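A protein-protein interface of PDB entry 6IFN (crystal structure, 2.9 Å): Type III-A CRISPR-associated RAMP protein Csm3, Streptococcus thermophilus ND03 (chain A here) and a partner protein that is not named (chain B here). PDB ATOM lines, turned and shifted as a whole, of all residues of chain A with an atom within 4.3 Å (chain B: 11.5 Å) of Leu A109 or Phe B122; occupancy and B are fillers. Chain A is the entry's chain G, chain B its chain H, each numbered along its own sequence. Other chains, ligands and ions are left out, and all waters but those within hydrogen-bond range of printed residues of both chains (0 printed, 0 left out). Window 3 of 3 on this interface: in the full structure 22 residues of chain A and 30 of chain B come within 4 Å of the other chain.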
ATOM      1  N   ASN A 105      41.081  26.698 -31.870  1.00  0.00           N
ATOM      2  CA  ASN A 105      40.880  25.247 -32.168  1.00  0.00           C
ATOM      3  C   ASN A 105      39.483  24.924 -32.734  1.00  0.00           C
ATOM      4  O   ASN A 105      39.005  23.786 -32.644  1.00  0.00           O
ATOM      5  CB  ASN A 105      41.125  24.416 -30.913  1.00  0.00           C
ATOM      6  CG  ASN A 105      40.185  24.783 -29.781  1.00  0.00           C
ATOM      7  OD1 ASN A 105      39.430  25.759 -29.871  1.00  0.00           O
ATOM      8  ND2 ASN A 105      40.226  23.999 -28.720  1.00  0.00           N
ATOM      9  N   ALA A 106      38.823  25.915 -33.336  1.00  0.00           N
ATOM     10  CA  ALA A 106      37.489  25.730 -33.945  1.00  0.00           C
ATOM     11  C   ALA A 106      37.415  24.410 -34.723  1.00  0.00           C
ATOM     12  O   ALA A 106      36.410  23.739 -34.690  1.00  0.00           O
ATOM     13  CB  ALA A 106      37.139  26.888 -34.845  1.00  0.00           C
ATOM     14  N   ASP A 107      38.481  24.058 -35.445  1.00  0.00           N
ATOM     15  CA  ASP A 107      38.505  22.850 -36.258  1.00  0.00           C
ATOM     16  C   ASP A 107      38.582  21.611 -35.362  1.00  0.00           C
ATOM     17  O   ASP A 107      37.845  20.666 -35.586  1.00  0.00           O
ATOM     18  CB  ASP A 107      39.611  22.951 -37.309  1.00  0.00           C
ATOM     19  CG  ASP A 107      39.282  23.985 -38.378  1.00  0.00           C
ATOM     20  OD1 ASP A 107      38.068  24.150 -38.681  1.00  0.00           O
ATOM     21  OD2 ASP A 107      40.226  24.633 -38.880  1.00  0.00           O
ATOM     22  N   GLU A 108      39.445  21.638 -34.344  1.00  0.00           N
ATOM     23  CA  GLU A 108      39.491  20.552 -33.350  1.00  0.00           C
ATOM     24  C   GLU A 108      38.069  20.268 -32.831  1.00  0.00           C
ATOM     25  O   GLU A 108      37.646  19.117 -32.729  1.00  0.00           O
ATOM     26  CB  GLU A 108      40.429  20.906 -32.194  1.00  0.00           C
ATOM     27  CG  GLU A 108      40.854  19.705 -31.357  1.00  0.00           C
ATOM     28  CD  GLU A 108      41.635  20.009 -30.085  1.00  0.00           C
ATOM     29  OE1 GLU A 108      41.676  21.173 -29.634  1.00  0.00           O
ATOM     30  OE2 GLU A 108      42.213  19.069 -29.533  1.00  0.00           O
ATOM     31  N   LEU A 109      37.332  21.332 -32.502  1.00  0.00           N
ATOM     32  CA  LEU A 109      35.999  21.208 -31.885  1.00  0.00           C
ATOM     33  C   LEU A 109      34.977  20.727 -32.922  1.00  0.00           C
ATOM     34  O   LEU A 109      34.120  19.926 -32.614  1.00  0.00           O
ATOM     35  CB  LEU A 109      35.584  22.553 -31.280  1.00  0.00           C
ATOM     36  CG  LEU A 109      36.510  23.073 -30.183  1.00  0.00           C
ATOM     37  CD1 LEU A 109      36.252  24.540 -29.888  1.00  0.00           C
ATOM     38  CD2 LEU A 109      36.350  22.240 -28.923  1.00  0.00           C
ATOM     39  N   ASP A 110      35.068  21.239 -34.145  1.00  0.00           N
ATOM     40  CA  ASP A 110      34.189  20.802 -35.205  1.00  0.00           C
ATOM     41  C   ASP A 110      34.359  19.289 -35.398  1.00  0.00           C
ATOM     42  O   ASP A 110      33.390  18.583 -35.647  1.00  0.00           O
ATOM     43  CB  ASP A 110      34.434  21.582 -36.498  1.00  0.00           C
ATOM     44  CG  ASP A 110      33.203  21.598 -37.388  1.00  0.00           C
ATOM     45  OD1 ASP A 110      32.301  22.410 -37.093  1.00  0.00           O
ATOM     46  OD2 ASP A 110      33.145  20.794 -38.351  1.00  0.00           O
ATOM     47  N   SER A 111      35.598  18.806 -35.260  1.00  0.00           N
ATOM     48  CA  SER A 111      35.908  17.370 -35.326  1.00  0.00           C
ATOM     49  C   SER A 111      35.270  16.618 -34.145  1.00  0.00           C
ATOM     50  O   SER A 111      34.721  15.542 -34.305  1.00  0.00           O
ATOM     51  CB  SER A 111      37.404  17.127 -35.378  1.00  0.00           C
ATOM     52  OG  SER A 111      37.789  16.090 -34.473  1.00  0.00           O
ATOM     53  N   LEU A 112      35.363  17.192 -32.946  1.00  0.00           N
ATOM     54  CA  LEU A 112      34.787  16.581 -31.732  1.00  0.00           C
ATOM     55  C   LEU A 112      33.244  16.642 -31.749  1.00  0.00           C
ATOM     56  O   LEU A 112      32.613  16.144 -30.840  1.00  0.00           O
ATOM     57  CB  LEU A 112      35.380  17.290 -30.509  1.00  0.00           C
ATOM     58  CG  LEU A 112      36.778  16.808 -30.124  1.00  0.00           C
ATOM     59  CD1 LEU A 112      37.387  17.676 -29.032  1.00  0.00           C
ATOM     60  CD2 LEU A 112      36.724  15.345 -29.720  1.00  0.00           C
ATOM     61  N   GLY A 113      32.652  17.279 -32.760  1.00  0.00           N
ATOM     62  CA  GLY A 113      31.227  17.124 -33.106  1.00  0.00           C
ATOM     63  C   GLY A 113      30.321  18.133 -32.430  1.00  0.00           C
ATOM     64  O   GLY A 113      29.166  17.824 -32.171  1.00  0.00           O
ATOM     65  N   VAL A 114      30.834  19.341 -32.176  1.00  0.00           N
ATOM     66  CA  VAL A 114      30.045  20.430 -31.576  1.00  0.00           C
ATOM     67  C   VAL A 114      29.119  21.024 -32.648  1.00  0.00           C
ATOM     68  O   VAL A 114      29.468  21.080 -33.808  1.00  0.00           O
ATOM     69  CB  VAL A 114      30.957  21.509 -30.960  1.00  0.00           C
ATOM     70  CG1 VAL A 114      31.884  20.926 -29.901  1.00  0.00           C
ATOM     71  CG2 VAL A 114      31.746  22.282 -32.014  1.00  0.00           C
ATOM     72  N   ILE A 142      32.665  27.473 -24.928  1.00  0.00           N
ATOM     73  CA  ILE A 142      32.568  26.063 -24.603  1.00  0.00           C
ATOM     74  C   ILE A 142      33.886  25.627 -23.982  1.00  0.00           C
ATOM     75  O   ILE A 142      34.930  26.234 -24.197  1.00  0.00           O
ATOM     76  CB  ILE A 142      32.168  25.180 -25.800  1.00  0.00           C
ATOM     77  CG1 ILE A 142      33.233  25.106 -26.890  1.00  0.00           C
ATOM     78  CG2 ILE A 142      30.825  25.604 -26.365  1.00  0.00           C
ATOM     79  CD1 ILE A 142      32.817  24.252 -28.082  1.00  0.00           C
ATOM     80  N   ARG A 143      33.786  24.555 -23.198  1.00  0.00           N
ATOM     81  CA  ARG A 143      34.887  23.965 -22.486  1.00  0.00           C
ATOM     82  C   ARG A 143      35.901  23.415 -23.501  1.00  0.00           C
ATOM     83  O   ARG A 143      35.538  23.012 -24.620  1.00  0.00           O
ATOM     84  CB  ARG A 143      34.300  22.890 -21.562  1.00  0.00           C
ATOM     85  CG  ARG A 143      35.295  22.214 -20.632  1.00  0.00           C
ATOM     86  CD  ARG A 143      34.707  20.935 -20.054  1.00  0.00           C
ATOM     87  NE  ARG A 143      35.762  19.981 -19.747  1.00  0.00           N
ATOM     88  CZ  ARG A 143      36.024  18.887 -20.455  1.00  0.00           C
ATOM     89  NH1 ARG A 143      35.180  18.485 -21.399  1.00  0.00           N
ATOM     90  NH2 ARG A 143      37.136  18.212 -20.221  1.00  0.00           N
ATOM     91  N   ASN A 144      37.174  23.427 -23.108  1.00  0.00           N
ATOM     92  CA  ASN A 144      38.300  22.905 -23.908  1.00  0.00           C
ATOM     93  C   ASN A 144      38.502  23.714 -25.193  1.00  0.00           C
ATOM     94  O   ASN A 144      39.168  23.241 -26.115  1.00  0.00           O
ATOM     95  CB  ASN A 144      38.149  21.419 -24.242  1.00  0.00           C
ATOM     96  CG  ASN A 144      38.881  20.499 -23.288  1.00  0.00           C
ATOM     97  OD1 ASN A 144      39.739  20.903 -22.496  1.00  0.00           O
ATOM     98  ND2 ASN A 144      38.586  19.220 -23.403  1.00  0.00           N
ATOM     99  N   SER A 145      37.947  24.936 -25.254  1.00  0.00           N
ATOM    100  CA  SER A 145      38.314  25.896 -26.269  1.00  0.00           C
ATOM    101  C   SER A 145      39.732  26.384 -25.963  1.00  0.00           C
ATOM    102  O   SER A 145      40.128  26.432 -24.795  1.00  0.00           O
ATOM    103  CB  SER A 145      37.341  27.028 -26.315  1.00  0.00           C
ATOM    104  OG  SER A 145      36.047  26.580 -26.667  1.00  0.00           O
ATOM    105  N   ASN B  22      19.111  19.040 -17.676  1.00  0.00           N
ATOM    106  CA  ASN B  22      18.833  20.296 -18.391  1.00  0.00           C
ATOM    107  C   ASN B  22      17.325  20.361 -18.660  1.00  0.00           C
ATOM    108  O   ASN B  22      16.561  19.663 -17.995  1.00  0.00           O
ATOM    109  CB  ASN B  22      19.684  20.374 -19.668  1.00  0.00           C
ATOM    110  CG  ASN B  22      19.489  19.196 -20.607  1.00  0.00           C
ATOM    111  OD1 ASN B  22      18.379  18.957 -21.083  1.00  0.00           O
ATOM    112  ND2 ASN B  22      20.554  18.449 -20.873  1.00  0.00           N
ATOM    113  N   TYR B  26      13.785  13.586 -24.207  1.00  0.00           N
ATOM    114  CA  TYR B  26      13.581  12.610 -25.308  1.00  0.00           C
ATOM    115  C   TYR B  26      12.124  12.154 -25.372  1.00  0.00           C
ATOM    116  O   TYR B  26      11.516  11.886 -24.342  1.00  0.00           O
ATOM    117  CB  TYR B  26      14.344  11.310 -25.100  1.00  0.00           C
ATOM    118  CG  TYR B  26      15.823  11.420 -24.862  1.00  0.00           C
ATOM    119  CD1 TYR B  26      16.691  11.779 -25.872  1.00  0.00           C
ATOM    120  CD2 TYR B  26      16.366  11.061 -23.642  1.00  0.00           C
ATOM    121  CE1 TYR B  26      18.063  11.812 -25.666  1.00  0.00           C
ATOM    122  CE2 TYR B  26      17.737  11.095 -23.415  1.00  0.00           C
ATOM    123  CZ  TYR B  26      18.596  11.462 -24.434  1.00  0.00           C
ATOM    124  OH  TYR B  26      19.944  11.464 -24.202  1.00  0.00           O
ATOM    125  N   PRO B  41      19.755   7.698 -30.941  1.00  0.00           N
ATOM    126  CA  PRO B  41      20.432   8.068 -32.176  1.00  0.00           C
ATOM    127  C   PRO B  41      20.799   9.559 -32.185  1.00  0.00           C
ATOM    128  O   PRO B  41      20.488  10.298 -31.243  1.00  0.00           O
ATOM    129  CB  PRO B  41      19.368   7.722 -33.232  1.00  0.00           C
ATOM    130  CG  PRO B  41      18.073   8.085 -32.552  1.00  0.00           C
ATOM    131  CD  PRO B  41      18.290   7.744 -31.085  1.00  0.00           C
ATOM    132  N   ASP B  42      21.464   9.979 -33.263  1.00  0.00           N
ATOM    133  CA  ASP B  42      21.598  11.362 -33.594  1.00  0.00           C
ATOM    134  C   ASP B  42      20.550  11.637 -34.670  1.00  0.00           C
ATOM    135  O   ASP B  42      20.708  11.162 -35.789  1.00  0.00           O
ATOM    136  CB  ASP B  42      23.024  11.679 -34.034  1.00  0.00           C
ATOM    137  CG  ASP B  42      23.258  13.165 -34.201  1.00  0.00           C
ATOM    138  OD1 ASP B  42      22.405  13.945 -33.755  1.00  0.00           O
ATOM    139  OD2 ASP B  42      24.285  13.534 -34.775  1.00  0.00           O
ATOM    140  N   GLY B  90      24.160   7.586 -34.822  1.00  0.00           N
ATOM    141  CA  GLY B  90      23.952   8.084 -33.453  1.00  0.00           C
ATOM    142  C   GLY B  90      24.885   7.364 -32.503  1.00  0.00           C
ATOM    143  O   GLY B  90      25.408   6.316 -32.885  1.00  0.00           O
ATOM    144  N   GLY B  91      25.105   7.916 -31.311  1.00  0.00           N
ATOM    145  CA  GLY B  91      26.042   7.281 -30.371  1.00  0.00           C
ATOM    146  C   GLY B  91      25.500   7.219 -28.964  1.00  0.00           C
ATOM    147  O   GLY B  91      24.559   7.954 -28.688  1.00  0.00           O
ATOM    148  N   TYR B  92      26.061   6.306 -28.166  1.00  0.00           N
ATOM    149  CA  TYR B  92      25.779   6.034 -26.734  1.00  0.00           C
ATOM    150  C   TYR B  92      24.344   5.568 -26.440  1.00  0.00           C
ATOM    151  O   TYR B  92      23.453   6.419 -26.337  1.00  0.00           O
ATOM    152  CB  TYR B  92      26.142   7.246 -25.923  1.00  0.00           C
ATOM    153  N   LYS B 116      16.201  14.168 -20.236  1.00  0.00           N
ATOM    154  CA  LYS B 116      17.637  14.122 -20.542  1.00  0.00           C
ATOM    155  C   LYS B 116      18.429  14.582 -19.323  1.00  0.00           C
ATOM    156  O   LYS B 116      18.039  15.561 -18.656  1.00  0.00           O
ATOM    157  CB  LYS B 116      17.992  15.083 -21.680  1.00  0.00           C
ATOM    158  CG  LYS B 116      17.682  14.625 -23.100  1.00  0.00           C
ATOM    159  CD  LYS B 116      17.808  15.746 -24.119  1.00  0.00           C
ATOM    160  CE  LYS B 116      18.377  15.300 -25.448  1.00  0.00           C
ATOM    161  NZ  LYS B 116      19.848  15.118 -25.394  1.00  0.00           N
ATOM    162  N   PHE B 117      19.566  13.929 -19.073  1.00  0.00           N
ATOM    163  CA  PHE B 117      20.522  14.463 -18.097  1.00  0.00           C
ATOM    164  C   PHE B 117      21.280  15.636 -18.732  1.00  0.00           C
ATOM    165  O   PHE B 117      21.385  15.685 -19.966  1.00  0.00           O
ATOM    166  CB  PHE B 117      21.479  13.376 -17.626  1.00  0.00           C
ATOM    167  CG  PHE B 117      22.267  13.750 -16.400  1.00  0.00           C
ATOM    168  CD1 PHE B 117      21.751  13.536 -15.137  1.00  0.00           C
ATOM    169  CD2 PHE B 117      23.516  14.329 -16.509  1.00  0.00           C
ATOM    170  CE1 PHE B 117      22.492  13.853 -14.007  1.00  0.00           C
ATOM    171  CE2 PHE B 117      24.249  14.664 -15.383  1.00  0.00           C
ATOM    172  CZ  PHE B 117      23.745  14.409 -14.131  1.00  0.00           C
ATOM    173  N   ILE B 118      21.794  16.561 -17.900  1.00  0.00           N
ATOM    174  CA  ILE B 118      22.451  17.787 -18.411  1.00  0.00           C
ATOM    175  C   ILE B 118      23.802  17.395 -19.020  1.00  0.00           C
ATOM    176  O   ILE B 118      24.676  16.837 -18.319  1.00  0.00           O
ATOM    177  CB  ILE B 118      22.656  18.888 -17.354  1.00  0.00           C
ATOM    178  CG1 ILE B 118      23.188  20.156 -18.034  1.00  0.00           C
ATOM    179  CG2 ILE B 118      23.587  18.414 -16.242  1.00  0.00           C
ATOM    180  CD1 ILE B 118      23.383  21.344 -17.125  1.00  0.00           C
ATOM    181  N   ARG B 119      23.971  17.704 -20.314  1.00  0.00           N
ATOM    182  CA  ARG B 119      25.182  17.331 -21.051  1.00  0.00           C
ATOM    183  C   ARG B 119      25.827  18.607 -21.603  1.00  0.00           C
ATOM    184  O   ARG B 119      25.148  19.583 -21.952  1.00  0.00           O
ATOM    185  CB  ARG B 119      24.886  16.285 -22.134  1.00  0.00           C
ATOM    186  CG  ARG B 119      23.839  15.253 -21.730  1.00  0.00           C
ATOM    187  CD  ARG B 119      24.047  13.849 -22.280  1.00  0.00           C
ATOM    188  NE  ARG B 119      22.797  13.091 -22.261  1.00  0.00           N
ATOM    189  CZ  ARG B 119      22.690  11.767 -22.385  1.00  0.00           C
ATOM    190  NH1 ARG B 119      21.490  11.197 -22.404  1.00  0.00           N
ATOM    191  NH2 ARG B 119      23.785  11.023 -22.472  1.00  0.00           N
ATOM    192  N   ASP B 120      27.158  18.565 -21.657  1.00  0.00           N
ATOM    193  CA  ASP B 120      27.985  19.690 -21.994  1.00  0.00           C
ATOM    194  C   ASP B 120      27.930  19.917 -23.514  1.00  0.00           C
ATOM    195  O   ASP B 120      27.092  19.333 -24.231  1.00  0.00           O
ATOM    196  CB  ASP B 120      29.392  19.471 -21.422  1.00  0.00           C
ATOM    197  CG  ASP B 120      30.314  18.573 -22.234  1.00  0.00           C
ATOM    198  OD1 ASP B 120      29.860  18.043 -23.273  1.00  0.00           O
ATOM    199  OD2 ASP B 120      31.506  18.449 -21.835  1.00  0.00           O
ATOM    200  N   ALA B 121      28.846  20.770 -23.989  1.00  0.00           N
ATOM    201  CA  ALA B 121      29.012  21.114 -25.406  1.00  0.00           C
ATOM    202  C   ALA B 121      29.128  19.865 -26.298  1.00  0.00           C
ATOM    203  O   ALA B 121      28.534  19.810 -27.395  1.00  0.00           O
ATOM    204  CB  ALA B 121      30.239  21.981 -25.536  1.00  0.00           C
ATOM    205  N   PHE B 122      29.882  18.874 -25.807  1.00  0.00           N
ATOM    206  CA  PHE B 122      30.379  17.768 -26.590  1.00  0.00           C
ATOM    207  C   PHE B 122      29.409  16.574 -26.640  1.00  0.00           C
ATOM    208  O   PHE B 122      29.558  15.697 -27.488  1.00  0.00           O
ATOM    209  CB  PHE B 122      31.719  17.334 -26.004  1.00  0.00           C
ATOM    210  CG  PHE B 122      32.804  18.377 -26.063  1.00  0.00           C
ATOM    211  CD1 PHE B 122      33.073  19.054 -27.240  1.00  0.00           C
ATOM    212  CD2 PHE B 122      33.600  18.633 -24.955  1.00  0.00           C
ATOM    213  CE1 PHE B 122      34.102  19.980 -27.301  1.00  0.00           C
ATOM    214  CE2 PHE B 122      34.625  19.561 -25.018  1.00  0.00           C
ATOM    215  CZ  PHE B 122      34.877  20.232 -26.192  1.00  0.00           C
ATOM    216  N   GLY B 123      28.426  16.519 -25.734  1.00  0.00           N
ATOM    217  CA  GLY B 123      27.443  15.410 -25.686  1.00  0.00           C
ATOM    218  C   GLY B 123      27.618  14.525 -24.462  1.00  0.00           C
ATOM    219  O   GLY B 123      26.737  13.757 -24.146  1.00  0.00           O
ATOM    220  N   ASN B 124      28.769  14.639 -23.787  1.00  0.00           N
ATOM    221  CA  ASN B 124      29.005  14.039 -22.467  1.00  0.00           C
ATOM    222  C   ASN B 124      28.147  14.758 -21.418  1.00  0.00           C
ATOM    223  O   ASN B 124      27.905  15.958 -21.534  1.00  0.00           O
ATOM    224  CB  ASN B 124      30.480  14.101 -22.037  1.00  0.00           C
ATOM    225  CG  ASN B 124      31.485  13.985 -23.170  1.00  0.00           C
ATOM    226  OD1 ASN B 124      31.530  12.967 -23.855  1.00  0.00           O
ATOM    227  ND2 ASN B 124      32.308  15.010 -23.357  1.00  0.00           N
ATOM    228  N   PRO B 125      27.663  14.068 -20.353  1.00  0.00           N
ATOM    229  CA  PRO B 125      27.029  14.729 -19.208  1.00  0.00           C
ATOM    230  C   PRO B 125      28.046  15.071 -18.106  1.00  0.00           C
ATOM    231  O   PRO B 125      29.172  14.551 -18.137  1.00  0.00           O
ATOM    232  CB  PRO B 125      26.013  13.687 -18.716  1.00  0.00           C
ATOM    233  CG  PRO B 125      26.356  12.378 -19.443  1.00  0.00           C
ATOM    234  CD  PRO B 125      27.656  12.608 -20.187  1.00  0.00           C
ATOM    235  N   TYR B 126      27.645  15.935 -17.162  1.00  0.00           N
ATOM    236  CA  TYR B 126      28.523  16.429 -16.071  1.00  0.00           C
ATOM    237  C   TYR B 126      27.659  17.015 -14.957  1.00  0.00           C
ATOM    238  O   TYR B 126      26.474  17.312 -15.178  1.00  0.00           O
ATOM    239  CB  TYR B 126      29.505  17.503 -16.562  1.00  0.00           C
ATOM    240  CG  TYR B 126      28.880  18.837 -16.907  1.00  0.00           C
ATOM    241  CD1 TYR B 126      27.975  18.963 -17.955  1.00  0.00           C
ATOM    242  CD2 TYR B 126      29.185  19.984 -16.186  1.00  0.00           C
ATOM    243  CE1 TYR B 126      27.380  20.178 -18.266  1.00  0.00           C
ATOM    244  CE2 TYR B 126      28.613  21.210 -16.494  1.00  0.00           C
ATOM    245  CZ  TYR B 126      27.707  21.308 -17.535  1.00  0.00           C
ATOM    246  OH  TYR B 126      27.152  22.513 -17.847  1.00  0.00           O
ATOM    247  N   ASP B 188      32.819  23.151 -11.539  1.00  0.00           N
ATOM    248  CA  ASP B 188      32.087  22.291 -12.447  1.00  0.00           C
ATOM    249  C   ASP B 188      32.775  20.930 -12.379  1.00  0.00           C
ATOM    250  O   ASP B 188      34.010  20.839 -12.213  1.00  0.00           O
ATOM    251  CB  ASP B 188      32.043  22.829 -13.884  1.00  0.00           C
ATOM    252  CG  ASP B 188      30.816  23.656 -14.260  1.00  0.00           C
ATOM    253  OD1 ASP B 188      29.966  23.944 -13.368  1.00  0.00           O
ATOM    254  OD2 ASP B 188      30.703  24.006 -15.459  1.00  0.00           O
ATOM    255  N   SER B 189      31.975  19.870 -12.465  1.00  0.00           N
ATOM    256  CA  SER B 189      32.542  18.545 -12.586  1.00  0.00           C
ATOM    257  C   SER B 189      33.288  18.430 -13.925  1.00  0.00           C
ATOM    258  O   SER B 189      33.093  19.240 -14.845  1.00  0.00           O
ATOM    259  CB  SER B 189      31.476  17.495 -12.465  1.00  0.00           C
ATOM    260  OG  SER B 189      32.026  16.281 -11.995  1.00  0.00           O
ATOM    261  N   LYS B 190      34.155  17.422 -14.028  1.00  0.00           N
ATOM    262  CA  LYS B 190      34.550  16.927 -15.322  1.00  0.00           C
ATOM    263  C   LYS B 190      33.318  16.304 -15.971  1.00  0.00           C
ATOM    264  O   LYS B 190      32.312  16.060 -15.313  1.00  0.00           O
ATOM    265  CB  LYS B 190      35.667  15.897 -15.174  1.00  0.00           C
ATOM    266  CG  LYS B 190      36.878  16.371 -14.379  1.00  0.00           C
ATOM    267  CD  LYS B 190      38.140  16.422 -15.200  1.00  0.00           C
ATOM    268  CE  LYS B 190      39.385  16.075 -14.411  1.00  0.00           C
ATOM    269  NZ  LYS B 190      40.034  17.286 -13.857  1.00  0.00           N
ATOM    270  N   PRO B 191      33.314  16.067 -17.294  1.00  0.00           N
ATOM    271  CA  PRO B 191      32.307  15.203 -17.892  1.00  0.00           C
ATOM    272  C   PRO B 191      32.694  13.774 -17.523  1.00  0.00           C
ATOM    273  O   PRO B 191      33.881  13.502 -17.349  1.00  0.00           O
ATOM    274  CB  PRO B 191      32.416  15.439 -19.398  1.00  0.00           C
ATOM    275  CG  PRO B 191      33.360  16.624 -19.547  1.00  0.00           C
ATOM    276  CD  PRO B 191      34.212  16.650 -18.293  1.00  0.00           C
ATOM    277  N   PHE B 192      31.697  12.898 -17.402  1.00  0.00           N
ATOM    278  CA  PHE B 192      31.936  11.476 -17.138  1.00  0.00           C
ATOM    279  C   PHE B 192      31.389  10.640 -18.308  1.00  0.00           C
ATOM    280  O   PHE B 192      30.533  11.099 -19.100  1.00  0.00           O
ATOM    281  CB  PHE B 192      31.353  11.068 -15.775  1.00  0.00           C
ATOM    282  CG  PHE B 192      29.894  11.406 -15.560  1.00  0.00           C
ATOM    283  CD1 PHE B 192      28.884  10.739 -16.247  1.00  0.00           C
ATOM    284  CD2 PHE B 192      29.523  12.400 -14.670  1.00  0.00           C
ATOM    285  CE1 PHE B 192      27.549  11.059 -16.048  1.00  0.00           C
ATOM    286  CE2 PHE B 192      28.187  12.717 -14.474  1.00  0.00           C
ATOM    287  CZ  PHE B 192      27.202  12.046 -15.161  1.00  0.00           C
ATOM    288  N   ASP B 193      31.882   9.398 -18.390  1.00  0.00           N
ATOM    289  CA  ASP B 193      31.499   8.445 -19.429  1.00  0.00           C
ATOM    290  C   ASP B 193      29.978   8.230 -19.381  1.00  0.00           C
ATOM    291  O   ASP B 193      29.440   7.814 -18.352  1.00  0.00           O
ATOM    292  CB  ASP B 193      32.252   7.120 -19.274  1.00  0.00           C
ATOM    293  CG  ASP B 193      32.296   6.292 -20.547  1.00  0.00           C
ATOM    294  OD1 ASP B 193      31.417   6.493 -21.414  1.00  0.00           O
ATOM    295  OD2 ASP B 193      33.211   5.458 -20.664  1.00  0.00           O
ATOM    296  N   ASN B 194      29.308   8.480 -20.516  1.00  0.00           N
ATOM    297  CA  ASN B 194      27.852   8.423 -20.609  1.00  0.00           C
ATOM    298  C   ASN B 194      27.348   6.997 -20.330  1.00  0.00           C
ATOM    299  O   ASN B 194      26.148   6.784 -20.308  1.00  0.00           O
ATOM    300  CB  ASN B 194      27.344   8.940 -21.962  1.00  0.00           C
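The side-chain carboxylate of Asp B120 is in salt-bridge range of the guanidinium group of Arg A143, at 3.7 Å.
OG of Ser A145 lies within hydrogen-bond range of O of Ile A142 (2.7 Å).
ND2 of Asn A105 sits at hydrogen-bond distance from O of Asn A144, 2.9 Å away.
OD1 of Asp B120 is in hydrogen-bond range of N of Gly B123 (3.2 Å).
N of Val A114 is in hydrogen-bond range of O of Leu A109 (3.4 Å).
The side-chain carboxylate of Asp B120 sits at hydrogen-bond distance from the backbone NH of Phe B122, 2.7 Å away.
Leu A109 touches Phe B122.
Phe B122 touches Val A114 (CD1 to CG1, 3.5 Å).
Ala B121 touches Ile A142.
O of Arg A143 touches CZ of Phe B122, at 3.3 Å.
CG of Pro B191 touches NH1 of Arg A143 (3.2 Å).
CZ of Phe B122 touches CB of Asn A144, at 3.99 Å.
No residue of chain B comes within 4 Å of Asn A105.
No residue of chain B comes within 4 Å of Ala A106.
No residue of chain B comes within 4 Å of Glu A108.
Of chain B, only Phe B122 comes within 4 Å of Leu A109.
No residue of chain B comes within 4 Å of Asp A110.
No residue of chain B comes within 4 Å of Leu A112.
No residue of chain B comes within 4 Å of Gly A113.
Arg A143 touches just these residues of chain B: Asp B120 (3.7 Å), Phe B122 (3.3 Å) and Pro B191 (3.2 Å).
Of the printed residues of chain B, Asn A144 touches Phe B122.
No residue of chain B comes within 4 Å of Ser A145.
Gly B91 touches none of the printed residues of chain A.
Of the printed residues of chain A, Ala B121 touches Ile A142.
Of the printed residues of chain A, Phe B122 touches Leu A109, Val A114, Arg A143 and Asn A144.
Printed residues of chain A within 4 Å of Pro B191: Arg A143.
Phe B192 touches none of the printed residues of chain A.
The nearest printed residue of chain A that does not touch Phe B122 is Leu A112 (4.4 Å).
The nearest printed residue of chain A that does not touch Pro B191 is Asn A144 (7.0 Å).
Of the 25 printed residues of chain B, 4 touch a printed residue of chain A.
Printed residues of chain B that touch a printed residue of chain A: Asp B120, Ala B121, Phe B122 and Pro B191.
Hydrophobic or aromatic side chains of chain B within 4 Å of the printed part of chain A: Ala B121, Phe B122 and Pro B191.
Of the 14 printed residues of chain A, 5 touch a printed residue of chain B.
Hydrophobic or aromatic side chains of chain A that line the printed part of chain B: Leu A109, Val A114 and Ile A142.
Among the printed residues, 7 pairs touch across the chains.
Among the printed residues, Asp or Glu carboxylates within 4 Å of a Lys or Arg side-chain nitrogen of the other chain: Arg A143 with Asp B120.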
